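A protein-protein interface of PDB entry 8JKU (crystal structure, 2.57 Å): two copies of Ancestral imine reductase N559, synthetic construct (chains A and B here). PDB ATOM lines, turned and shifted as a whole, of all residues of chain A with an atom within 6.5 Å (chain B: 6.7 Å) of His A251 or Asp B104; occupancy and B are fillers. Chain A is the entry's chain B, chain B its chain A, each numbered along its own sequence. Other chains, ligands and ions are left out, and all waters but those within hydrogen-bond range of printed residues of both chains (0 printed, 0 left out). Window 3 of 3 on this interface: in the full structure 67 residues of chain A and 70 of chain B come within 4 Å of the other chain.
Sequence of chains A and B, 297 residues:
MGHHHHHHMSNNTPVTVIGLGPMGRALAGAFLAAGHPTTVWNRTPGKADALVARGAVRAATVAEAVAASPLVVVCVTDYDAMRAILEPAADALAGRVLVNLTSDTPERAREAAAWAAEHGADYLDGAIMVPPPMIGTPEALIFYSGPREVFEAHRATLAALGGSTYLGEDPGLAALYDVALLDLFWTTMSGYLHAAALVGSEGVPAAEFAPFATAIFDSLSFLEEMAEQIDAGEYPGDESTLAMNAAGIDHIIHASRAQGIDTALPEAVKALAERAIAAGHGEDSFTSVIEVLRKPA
A ring nitrogen (NE2) of His A251 sits at hydrogen-bond distance from the side-chain carboxylate (OD1) of Asp B104, at 3.2 Å.
The backbone NH (N) of Tyr B79 sits at hydrogen-bond distance from the side-chain carboxylate (OD2) of Asp B104 (3.2 Å). OG of Ser B103 lies within hydrogen-bond range of OD2 of Asp B178 (2.8 Å). OD1 of Asp B104 lies within hydrogen-bond range of OG1 of Thr B105. The backbone NH (N) of Arg B108 lies within hydrogen-bond range of the side-chain hydroxyl (OG1) of Thr B105 (3.3 Å). A ring nitrogen (ND1) of His A251 sits at hydrogen-bond distance from the backbone carbonyl oxygen (O) of Ala A247 (3.5 Å). The backbone carbonyl oxygen (O) of Ile A252 is in hydrogen-bond range of the side-chain hydroxyl (OG) of Ser A256, 2.8 Å away.
His A251 touches Ser B103 (CE1 to O, 3.98 Å). Thr B105 touches His A251 (CG2 to CD2, 3.6 Å). O of Val B179 touches CG1 of Ile A252, at 3.4 Å. Pro B106 touches Ala A255 (CD to CB, 3.7 Å).
Of chain B, only Ser B103, Asp B104 and Thr B105 come within 4 Å of His A251. Printed residues of chain B within 4 Å of Ile A252: Val B179 (3.4 Å). Of the printed residues of chain B, Ala A255 touches Pro B106. Of the printed residues of chain A, Ser B103 touches His A251. Asp B104 touches one residue of chain A. Arg B108 touches none of the printed residues of chain A. Ala B175 touches none of the printed residues of chain A. The nearest printed residue of chain A that does not touch Asp B104 is Ala A255 (6.6 Å).
Of the 11 printed residues of chain A, 3 touch a printed residue of chain B. Among the printed residues, no Asp or Glu carboxylate lies within 4 Å of a Lys or Arg side-chain nitrogen of the other chain.
No position is printed for both chains. Of the 5 pairs that touch across the chains among the printed residues, none has its exchanged pair printed and touching as well.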
ATOM      1  N   ALA A 246      -9.039  10.100 -16.348  1.00  0.00           N
ATOM      2  CA  ALA A 246      -8.056  10.520 -15.357  1.00  0.00           C
ATOM      3  C   ALA A 246      -7.153  11.617 -15.908  1.00  0.00           C
ATOM      4  O   ALA A 246      -6.746  12.523 -15.171  1.00  0.00           O
ATOM      5  CB  ALA A 246      -7.228   9.320 -14.900  1.00  0.00           C
ATOM      6  N   ALA A 247      -6.829  11.551 -17.202  1.00  0.00           N
ATOM      7  CA  ALA A 247      -5.988  12.584 -17.801  1.00  0.00           C
ATOM      8  C   ALA A 247      -6.696  13.931 -17.832  1.00  0.00           C
ATOM      9  O   ALA A 247      -6.047  14.975 -17.699  1.00  0.00           O
ATOM     10  CB  ALA A 247      -5.574  12.178 -19.215  1.00  0.00           C
ATOM     11  N   GLY A 248      -8.017  13.929 -18.016  1.00  0.00           N
ATOM     12  CA  GLY A 248      -8.762  15.173 -17.930  1.00  0.00           C
ATOM     13  C   GLY A 248      -8.801  15.723 -16.518  1.00  0.00           C
ATOM     14  O   GLY A 248      -8.720  16.937 -16.311  1.00  0.00           O
ATOM     15  N   ILE A 249      -8.926  14.839 -15.525  1.00  0.00           N
ATOM     16  CA  ILE A 249      -8.889  15.280 -14.136  1.00  0.00           C
ATOM     17  C   ILE A 249      -7.528  15.876 -13.808  1.00  0.00           C
ATOM     18  O   ILE A 249      -7.423  16.789 -12.980  1.00  0.00           O
ATOM     19  CB  ILE A 249      -9.245  14.111 -13.197  1.00  0.00           C
ATOM     20  CG1 ILE A 249     -10.714  13.723 -13.380  1.00  0.00           C
ATOM     21  CG2 ILE A 249      -8.972  14.486 -11.747  1.00  0.00           C
ATOM     22  CD1 ILE A 249     -10.985  12.245 -13.217  1.00  0.00           C
ATOM     23  N   ASP A 250      -6.467  15.377 -14.450  1.00  0.00           N
ATOM     24  CA  ASP A 250      -5.162  16.013 -14.312  1.00  0.00           C
ATOM     25  C   ASP A 250      -5.195  17.439 -14.846  1.00  0.00           C
ATOM     26  O   ASP A 250      -4.638  18.357 -14.230  1.00  0.00           O
ATOM     27  CB  ASP A 250      -4.098  15.200 -15.046  1.00  0.00           C
ATOM     28  CG  ASP A 250      -3.251  14.364 -14.107  1.00  0.00           C
ATOM     29  OD1 ASP A 250      -2.703  14.928 -13.136  1.00  0.00           O
ATOM     30  OD2 ASP A 250      -3.132  13.144 -14.343  1.00  0.00           O
ATOM     31  N   HIS A 251      -5.844  17.643 -15.995  1.00  0.00           N
ATOM     32  CA  HIS A 251      -5.958  18.987 -16.551  1.00  0.00           C
ATOM     33  C   HIS A 251      -6.731  19.903 -15.611  1.00  0.00           C
ATOM     34  O   HIS A 251      -6.406  21.090 -15.480  1.00  0.00           O
ATOM     35  CB  HIS A 251      -6.635  18.930 -17.921  1.00  0.00           C
ATOM     36  CG  HIS A 251      -5.782  18.326 -18.992  1.00  0.00           C
ATOM     37  ND1 HIS A 251      -6.300  17.558 -20.013  1.00  0.00           N
ATOM     38  CD2 HIS A 251      -4.445  18.381 -19.203  1.00  0.00           C
ATOM     39  CE1 HIS A 251      -5.319  17.164 -20.805  1.00  0.00           C
ATOM     40  NE2 HIS A 251      -4.184  17.649 -20.337  1.00  0.00           N
ATOM     41  N   ILE A 252      -7.760  19.370 -14.947  1.00  0.00           N
ATOM     42  CA  ILE A 252      -8.530  20.176 -14.004  1.00  0.00           C
ATOM     43  C   ILE A 252      -7.643  20.635 -12.857  1.00  0.00           C
ATOM     44  O   ILE A 252      -7.722  21.786 -12.411  1.00  0.00           O
ATOM     45  CB  ILE A 252      -9.744  19.380 -13.492  1.00  0.00           C
ATOM     46  CG1 ILE A 252     -10.737  19.130 -14.629  1.00  0.00           C
ATOM     47  CG2 ILE A 252     -10.427  20.117 -12.349  1.00  0.00           C
ATOM     48  CD1 ILE A 252     -11.577  17.888 -14.438  1.00  0.00           C
ATOM     49  N   ILE A 253      -6.783  19.744 -12.362  1.00  0.00           N
ATOM     50  CA  ILE A 253      -5.913  20.093 -11.244  1.00  0.00           C
ATOM     51  C   ILE A 253      -4.868  21.111 -11.682  1.00  0.00           C
ATOM     52  O   ILE A 253      -4.687  22.154 -11.044  1.00  0.00           O
ATOM     53  CB  ILE A 253      -5.256  18.828 -10.662  1.00  0.00           C
ATOM     54  CG1 ILE A 253      -6.308  17.916 -10.031  1.00  0.00           C
ATOM     55  CG2 ILE A 253      -4.205  19.204  -9.629  1.00  0.00           C
ATOM     56  CD1 ILE A 253      -5.903  16.456  -9.986  1.00  0.00           C
ATOM     57  N   HIS A 254      -4.163  20.824 -12.779  1.00  0.00           N
ATOM     58  CA  HIS A 254      -3.140  21.750 -13.253  1.00  0.00           C
ATOM     59  C   HIS A 254      -3.743  23.108 -13.584  1.00  0.00           C
ATOM     60  O   HIS A 254      -3.154  24.151 -13.273  1.00  0.00           O
ATOM     61  CB  HIS A 254      -2.428  21.163 -14.471  1.00  0.00           C
ATOM     62  CG  HIS A 254      -1.776  19.840 -14.210  1.00  0.00           C
ATOM     63  ND1 HIS A 254      -1.446  18.961 -15.220  1.00  0.00           N
ATOM     64  CD2 HIS A 254      -1.395  19.246 -13.055  1.00  0.00           C
ATOM     65  CE1 HIS A 254      -0.890  17.883 -14.696  1.00  0.00           C
ATOM     66  NE2 HIS A 254      -0.846  18.031 -13.385  1.00  0.00           N
ATOM     67  N   ALA A 255      -4.924  23.119 -14.203  1.00  0.00           N
ATOM     68  CA  ALA A 255      -5.574  24.386 -14.519  1.00  0.00           C
ATOM     69  C   ALA A 255      -5.995  25.122 -13.254  1.00  0.00           C
ATOM     70  O   ALA A 255      -5.787  26.334 -13.137  1.00  0.00           O
ATOM     71  CB  ALA A 255      -6.780  24.146 -15.428  1.00  0.00           C
ATOM     72  N   SER A 256      -6.592  24.407 -12.295  1.00  0.00           N
ATOM     73  CA  SER A 256      -7.010  25.048 -11.052  1.00  0.00           C
ATOM     74  C   SER A 256      -5.818  25.645 -10.315  1.00  0.00           C
ATOM     75  O   SER A 256      -5.882  26.781  -9.827  1.00  0.00           O
ATOM     76  CB  SER A 256      -7.739  24.040 -10.163  1.00  0.00           C
ATOM     77  OG  SER A 256      -8.977  23.659 -10.742  1.00  0.00           O
ATOM     78  N   THR B  77      -5.283  13.945 -29.218  1.00  0.00           N
ATOM     79  CA  THR B  77      -5.493  13.629 -27.807  1.00  0.00           C
ATOM     80  C   THR B  77      -5.190  14.828 -26.915  1.00  0.00           C
ATOM     81  O   THR B  77      -6.047  15.280 -26.148  1.00  0.00           O
ATOM     82  CB  THR B  77      -4.627  12.431 -27.406  1.00  0.00           C
ATOM     83  OG1 THR B  77      -5.143  11.238 -28.007  1.00  0.00           O
ATOM     84  CG2 THR B  77      -4.613  12.264 -25.894  1.00  0.00           C
ATOM     85  N   ASP B  78      -3.964  15.338 -26.982  1.00  0.00           N
ATOM     86  CA  ASP B  78      -3.537  16.480 -26.188  1.00  0.00           C
ATOM     87  C   ASP B  78      -2.804  17.458 -27.097  1.00  0.00           C
ATOM     88  O   ASP B  78      -2.644  17.222 -28.299  1.00  0.00           O
ATOM     89  CB  ASP B  78      -2.641  16.041 -25.021  1.00  0.00           C
ATOM     90  CG  ASP B  78      -1.720  14.893 -25.391  1.00  0.00           C
ATOM     91  OD1 ASP B  78      -1.405  14.748 -26.592  1.00  0.00           O
ATOM     92  OD2 ASP B  78      -1.313  14.138 -24.484  1.00  0.00           O
ATOM     93  N   TYR B  79      -2.352  18.571 -26.519  1.00  0.00           N
ATOM     94  CA  TYR B  79      -1.599  19.534 -27.312  1.00  0.00           C
ATOM     95  C   TYR B  79      -0.182  19.038 -27.586  1.00  0.00           C
ATOM     96  O   TYR B  79       0.406  19.388 -28.615  1.00  0.00           O
ATOM     97  CB  TYR B  79      -1.561  20.886 -26.608  1.00  0.00           C
ATOM     98  CG  TYR B  79      -2.832  21.693 -26.711  1.00  0.00           C
ATOM     99  CD1 TYR B  79      -4.074  21.077 -26.687  1.00  0.00           C
ATOM    100  CD2 TYR B  79      -2.788  23.075 -26.824  1.00  0.00           C
ATOM    101  CE1 TYR B  79      -5.241  21.816 -26.769  1.00  0.00           C
ATOM    102  CE2 TYR B  79      -3.947  23.823 -26.908  1.00  0.00           C
ATOM    103  CZ  TYR B  79      -5.171  23.189 -26.879  1.00  0.00           C
ATOM    104  OH  TYR B  79      -6.326  23.932 -26.968  1.00  0.00           O
ATOM    105  N   ASP B  80       0.384  18.236 -26.680  1.00  0.00           N
ATOM    106  CA  ASP B  80       1.678  17.618 -26.952  1.00  0.00           C
ATOM    107  C   ASP B  80       1.652  16.880 -28.282  1.00  0.00           C
ATOM    108  O   ASP B  80       2.627  16.907 -29.041  1.00  0.00           O
ATOM    109  CB  ASP B  80       2.057  16.661 -25.822  1.00  0.00           C
ATOM    110  CG  ASP B  80       2.392  17.384 -24.532  1.00  0.00           C
ATOM    111  OD1 ASP B  80       2.966  18.492 -24.600  1.00  0.00           O
ATOM    112  OD2 ASP B  80       2.082  16.840 -23.451  1.00  0.00           O
ATOM    113  N   THR B 102      -8.656  20.258 -29.798  1.00  0.00           N
ATOM    114  CA  THR B 102      -8.090  19.342 -28.820  1.00  0.00           C
ATOM    115  C   THR B 102      -8.335  19.885 -27.418  1.00  0.00           C
ATOM    116  O   THR B 102      -8.243  21.093 -27.181  1.00  0.00           O
ATOM    117  CB  THR B 102      -6.593  19.157 -29.066  1.00  0.00           C
ATOM    118  OG1 THR B 102      -6.383  18.662 -30.396  1.00  0.00           O
ATOM    119  CG2 THR B 102      -6.002  18.180 -28.059  1.00  0.00           C
ATOM    120  N   SER B 103      -8.660  18.990 -26.491  1.00  0.00           N
ATOM    121  CA  SER B 103      -8.992  19.376 -25.125  1.00  0.00           C
ATOM    122  C   SER B 103      -7.728  19.379 -24.273  1.00  0.00           C
ATOM    123  O   SER B 103      -7.025  18.365 -24.193  1.00  0.00           O
ATOM    124  CB  SER B 103     -10.033  18.426 -24.534  1.00  0.00           C
ATOM    125  OG  SER B 103     -11.351  18.877 -24.796  1.00  0.00           O
ATOM    126  N   ASP B 104      -7.444  20.510 -23.636  1.00  0.00           N
ATOM    127  CA  ASP B 104      -6.291  20.625 -22.750  1.00  0.00           C
ATOM    128  C   ASP B 104      -6.496  21.837 -21.844  1.00  0.00           C
ATOM    129  O   ASP B 104      -7.602  22.377 -21.740  1.00  0.00           O
ATOM    130  CB  ASP B 104      -4.992  20.714 -23.560  1.00  0.00           C
ATOM    131  CG  ASP B 104      -3.847  19.955 -22.915  1.00  0.00           C
ATOM    132  OD1 ASP B 104      -3.396  20.370 -21.825  1.00  0.00           O
ATOM    133  OD2 ASP B 104      -3.399  18.944 -23.496  1.00  0.00           O
ATOM    134  N   THR B 105      -5.424  22.267 -21.188  1.00  0.00           N
ATOM    135  CA  THR B 105      -5.513  23.314 -20.183  1.00  0.00           C
ATOM    136  C   THR B 105      -5.584  24.697 -20.822  1.00  0.00           C
ATOM    137  O   THR B 105      -5.141  24.893 -21.956  1.00  0.00           O
ATOM    138  CB  THR B 105      -4.307  23.251 -19.252  1.00  0.00           C
ATOM    139  OG1 THR B 105      -3.106  23.352 -20.027  1.00  0.00           O
ATOM    140  CG2 THR B 105      -4.299  21.947 -18.468  1.00  0.00           C
ATOM    141  N   PRO B 106      -6.145  25.678 -20.107  1.00  0.00           N
ATOM    142  CA  PRO B 106      -6.133  27.054 -20.637  1.00  0.00           C
ATOM    143  C   PRO B 106      -4.736  27.561 -20.950  1.00  0.00           C
ATOM    144  O   PRO B 106      -4.553  28.308 -21.921  1.00  0.00           O
ATOM    145  CB  PRO B 106      -6.798  27.866 -19.516  1.00  0.00           C
ATOM    146  CG  PRO B 106      -7.677  26.877 -18.807  1.00  0.00           C
ATOM    147  CD  PRO B 106      -6.939  25.561 -18.868  1.00  0.00           C
ATOM    148  N   GLU B 107      -3.740  27.182 -20.146  1.00  0.00           N
ATOM    149  CA  GLU B 107      -2.369  27.597 -20.423  1.00  0.00           C
ATOM    150  C   GLU B 107      -1.897  27.060 -21.769  1.00  0.00           C
ATOM    151  O   GLU B 107      -1.276  27.786 -22.553  1.00  0.00           O
ATOM    152  CB  GLU B 107      -1.450  27.132 -19.291  1.00  0.00           C
ATOM    153  CG  GLU B 107       0.039  27.209 -19.587  1.00  0.00           C
ATOM    154  CD  GLU B 107       0.837  26.166 -18.814  1.00  0.00           C
ATOM    155  OE1 GLU B 107       0.763  24.973 -19.177  1.00  0.00           O
ATOM    156  OE2 GLU B 107       1.532  26.539 -17.843  1.00  0.00           O
ATOM    157  N   ARG B 108      -2.172  25.785 -22.051  1.00  0.00           N
ATOM    158  CA  ARG B 108      -1.729  25.208 -23.315  1.00  0.00           C
ATOM    159  C   ARG B 108      -2.445  25.844 -24.501  1.00  0.00           C
ATOM    160  O   ARG B 108      -1.866  25.945 -25.588  1.00  0.00           O
ATOM    161  CB  ARG B 108      -1.943  23.694 -23.301  1.00  0.00           C
ATOM    162  CG  ARG B 108      -0.919  22.913 -22.471  1.00  0.00           C
ATOM    163  CD  ARG B 108       0.511  23.037 -23.012  1.00  0.00           C
ATOM    164  NE  ARG B 108       0.564  23.555 -24.376  1.00  0.00           N
ATOM    165  CZ  ARG B 108       0.730  22.810 -25.459  1.00  0.00           C
ATOM    166  NH1 ARG B 108       0.911  21.501 -25.377  1.00  0.00           N
ATOM    167  NH2 ARG B 108       0.723  23.395 -26.655  1.00  0.00           N
ATOM    168  N   ALA B 109      -3.692  26.285 -24.317  1.00  0.00           N
ATOM    169  CA  ALA B 109      -4.384  26.990 -25.391  1.00  0.00           C
ATOM    170  C   ALA B 109      -3.728  28.336 -25.673  1.00  0.00           C
ATOM    171  O   ALA B 109      -3.665  28.774 -26.829  1.00  0.00           O
ATOM    172  CB  ALA B 109      -5.858  27.180 -25.033  1.00  0.00           C
ATOM    173  N   ASP B 125      -9.276  28.699 -30.344  1.00  0.00           N
ATOM    174  CA  ASP B 125      -9.294  27.562 -29.438  1.00  0.00           C
ATOM    175  C   ASP B 125     -10.731  27.106 -29.237  1.00  0.00           C
ATOM    176  O   ASP B 125     -11.610  27.921 -28.939  1.00  0.00           O
ATOM    177  CB  ASP B 125      -8.660  27.920 -28.096  1.00  0.00           C
ATOM    178  CG  ASP B 125      -8.339  26.697 -27.266  1.00  0.00           C
ATOM    179  OD1 ASP B 125      -7.420  25.941 -27.651  1.00  0.00           O
ATOM    180  OD2 ASP B 125      -9.008  26.489 -26.231  1.00  0.00           O
ATOM    181  N   GLY B 126     -10.966  25.805 -29.405  1.00  0.00           N
ATOM    182  CA  GLY B 126     -12.288  25.248 -29.246  1.00  0.00           C
ATOM    183  C   GLY B 126     -12.277  24.082 -28.275  1.00  0.00           C
ATOM    184  O   GLY B 126     -11.244  23.463 -28.015  1.00  0.00           O
ATOM    185  N   ALA B 174     -12.209  28.983 -23.686  1.00  0.00           N
ATOM    186  CA  ALA B 174     -12.881  27.742 -24.061  1.00  0.00           C
ATOM    187  C   ALA B 174     -12.376  26.571 -23.229  1.00  0.00           C
ATOM    188  O   ALA B 174     -13.169  25.765 -22.729  1.00  0.00           O
ATOM    189  CB  ALA B 174     -12.681  27.466 -25.553  1.00  0.00           C
ATOM    190  N   ALA B 175     -11.056  26.470 -23.056  1.00  0.00           N
ATOM    191  CA  ALA B 175     -10.500  25.407 -22.226  1.00  0.00           C
ATOM    192  C   ALA B 175     -10.918  25.567 -20.768  1.00  0.00           C
ATOM    193  O   ALA B 175     -11.162  24.571 -20.076  1.00  0.00           O
ATOM    194  CB  ALA B 175      -8.976  25.389 -22.351  1.00  0.00           C
ATOM    195  N   LEU B 176     -11.009  26.810 -20.285  1.00  0.00           N
ATOM    196  CA  LEU B 176     -11.423  27.038 -18.903  1.00  0.00           C
ATOM    197  C   LEU B 176     -12.842  26.536 -18.669  1.00  0.00           C
ATOM    198  O   LEU B 176     -13.106  25.810 -17.705  1.00  0.00           O
ATOM    199  CB  LEU B 176     -11.317  28.524 -18.559  1.00  0.00           C
ATOM    200  CG  LEU B 176     -11.559  28.878 -17.088  1.00  0.00           C
ATOM    201  CD1 LEU B 176     -10.526  28.213 -16.190  1.00  0.00           C
ATOM    202  CD2 LEU B 176     -11.553  30.388 -16.882  1.00  0.00           C
ATOM    203  N   ASP B 178     -14.157  24.305 -20.352  1.00  0.00           N
ATOM    204  CA  ASP B 178     -14.095  22.862 -20.556  1.00  0.00           C
ATOM    205  C   ASP B 178     -13.684  22.146 -19.278  1.00  0.00           C
ATOM    206  O   ASP B 178     -14.371  21.223 -18.825  1.00  0.00           O
ATOM    207  CB  ASP B 178     -13.126  22.546 -21.696  1.00  0.00           C
ATOM    208  CG  ASP B 178     -13.207  21.101 -22.151  1.00  0.00           C
ATOM    209  OD1 ASP B 178     -14.215  20.429 -21.849  1.00  0.00           O
ATOM    210  OD2 ASP B 178     -12.259  20.637 -22.817  1.00  0.00           O
ATOM    211  N   VAL B 179     -12.567  22.558 -18.675  1.00  0.00           N
ATOM    212  CA  VAL B 179     -12.120  21.893 -17.454  1.00  0.00           C
ATOM    213  C   VAL B 179     -13.084  22.171 -16.308  1.00  0.00           C
ATOM    214  O   VAL B 179     -13.255  21.331 -15.414  1.00  0.00           O
ATOM    215  CB  VAL B 179     -10.685  22.322 -17.094  1.00  0.00           C
ATOM    216  CG1 VAL B 179      -9.716  21.851 -18.165  1.00  0.00           C
ATOM    217  CG2 VAL B 179     -10.601  23.831 -16.912  1.00  0.00           C
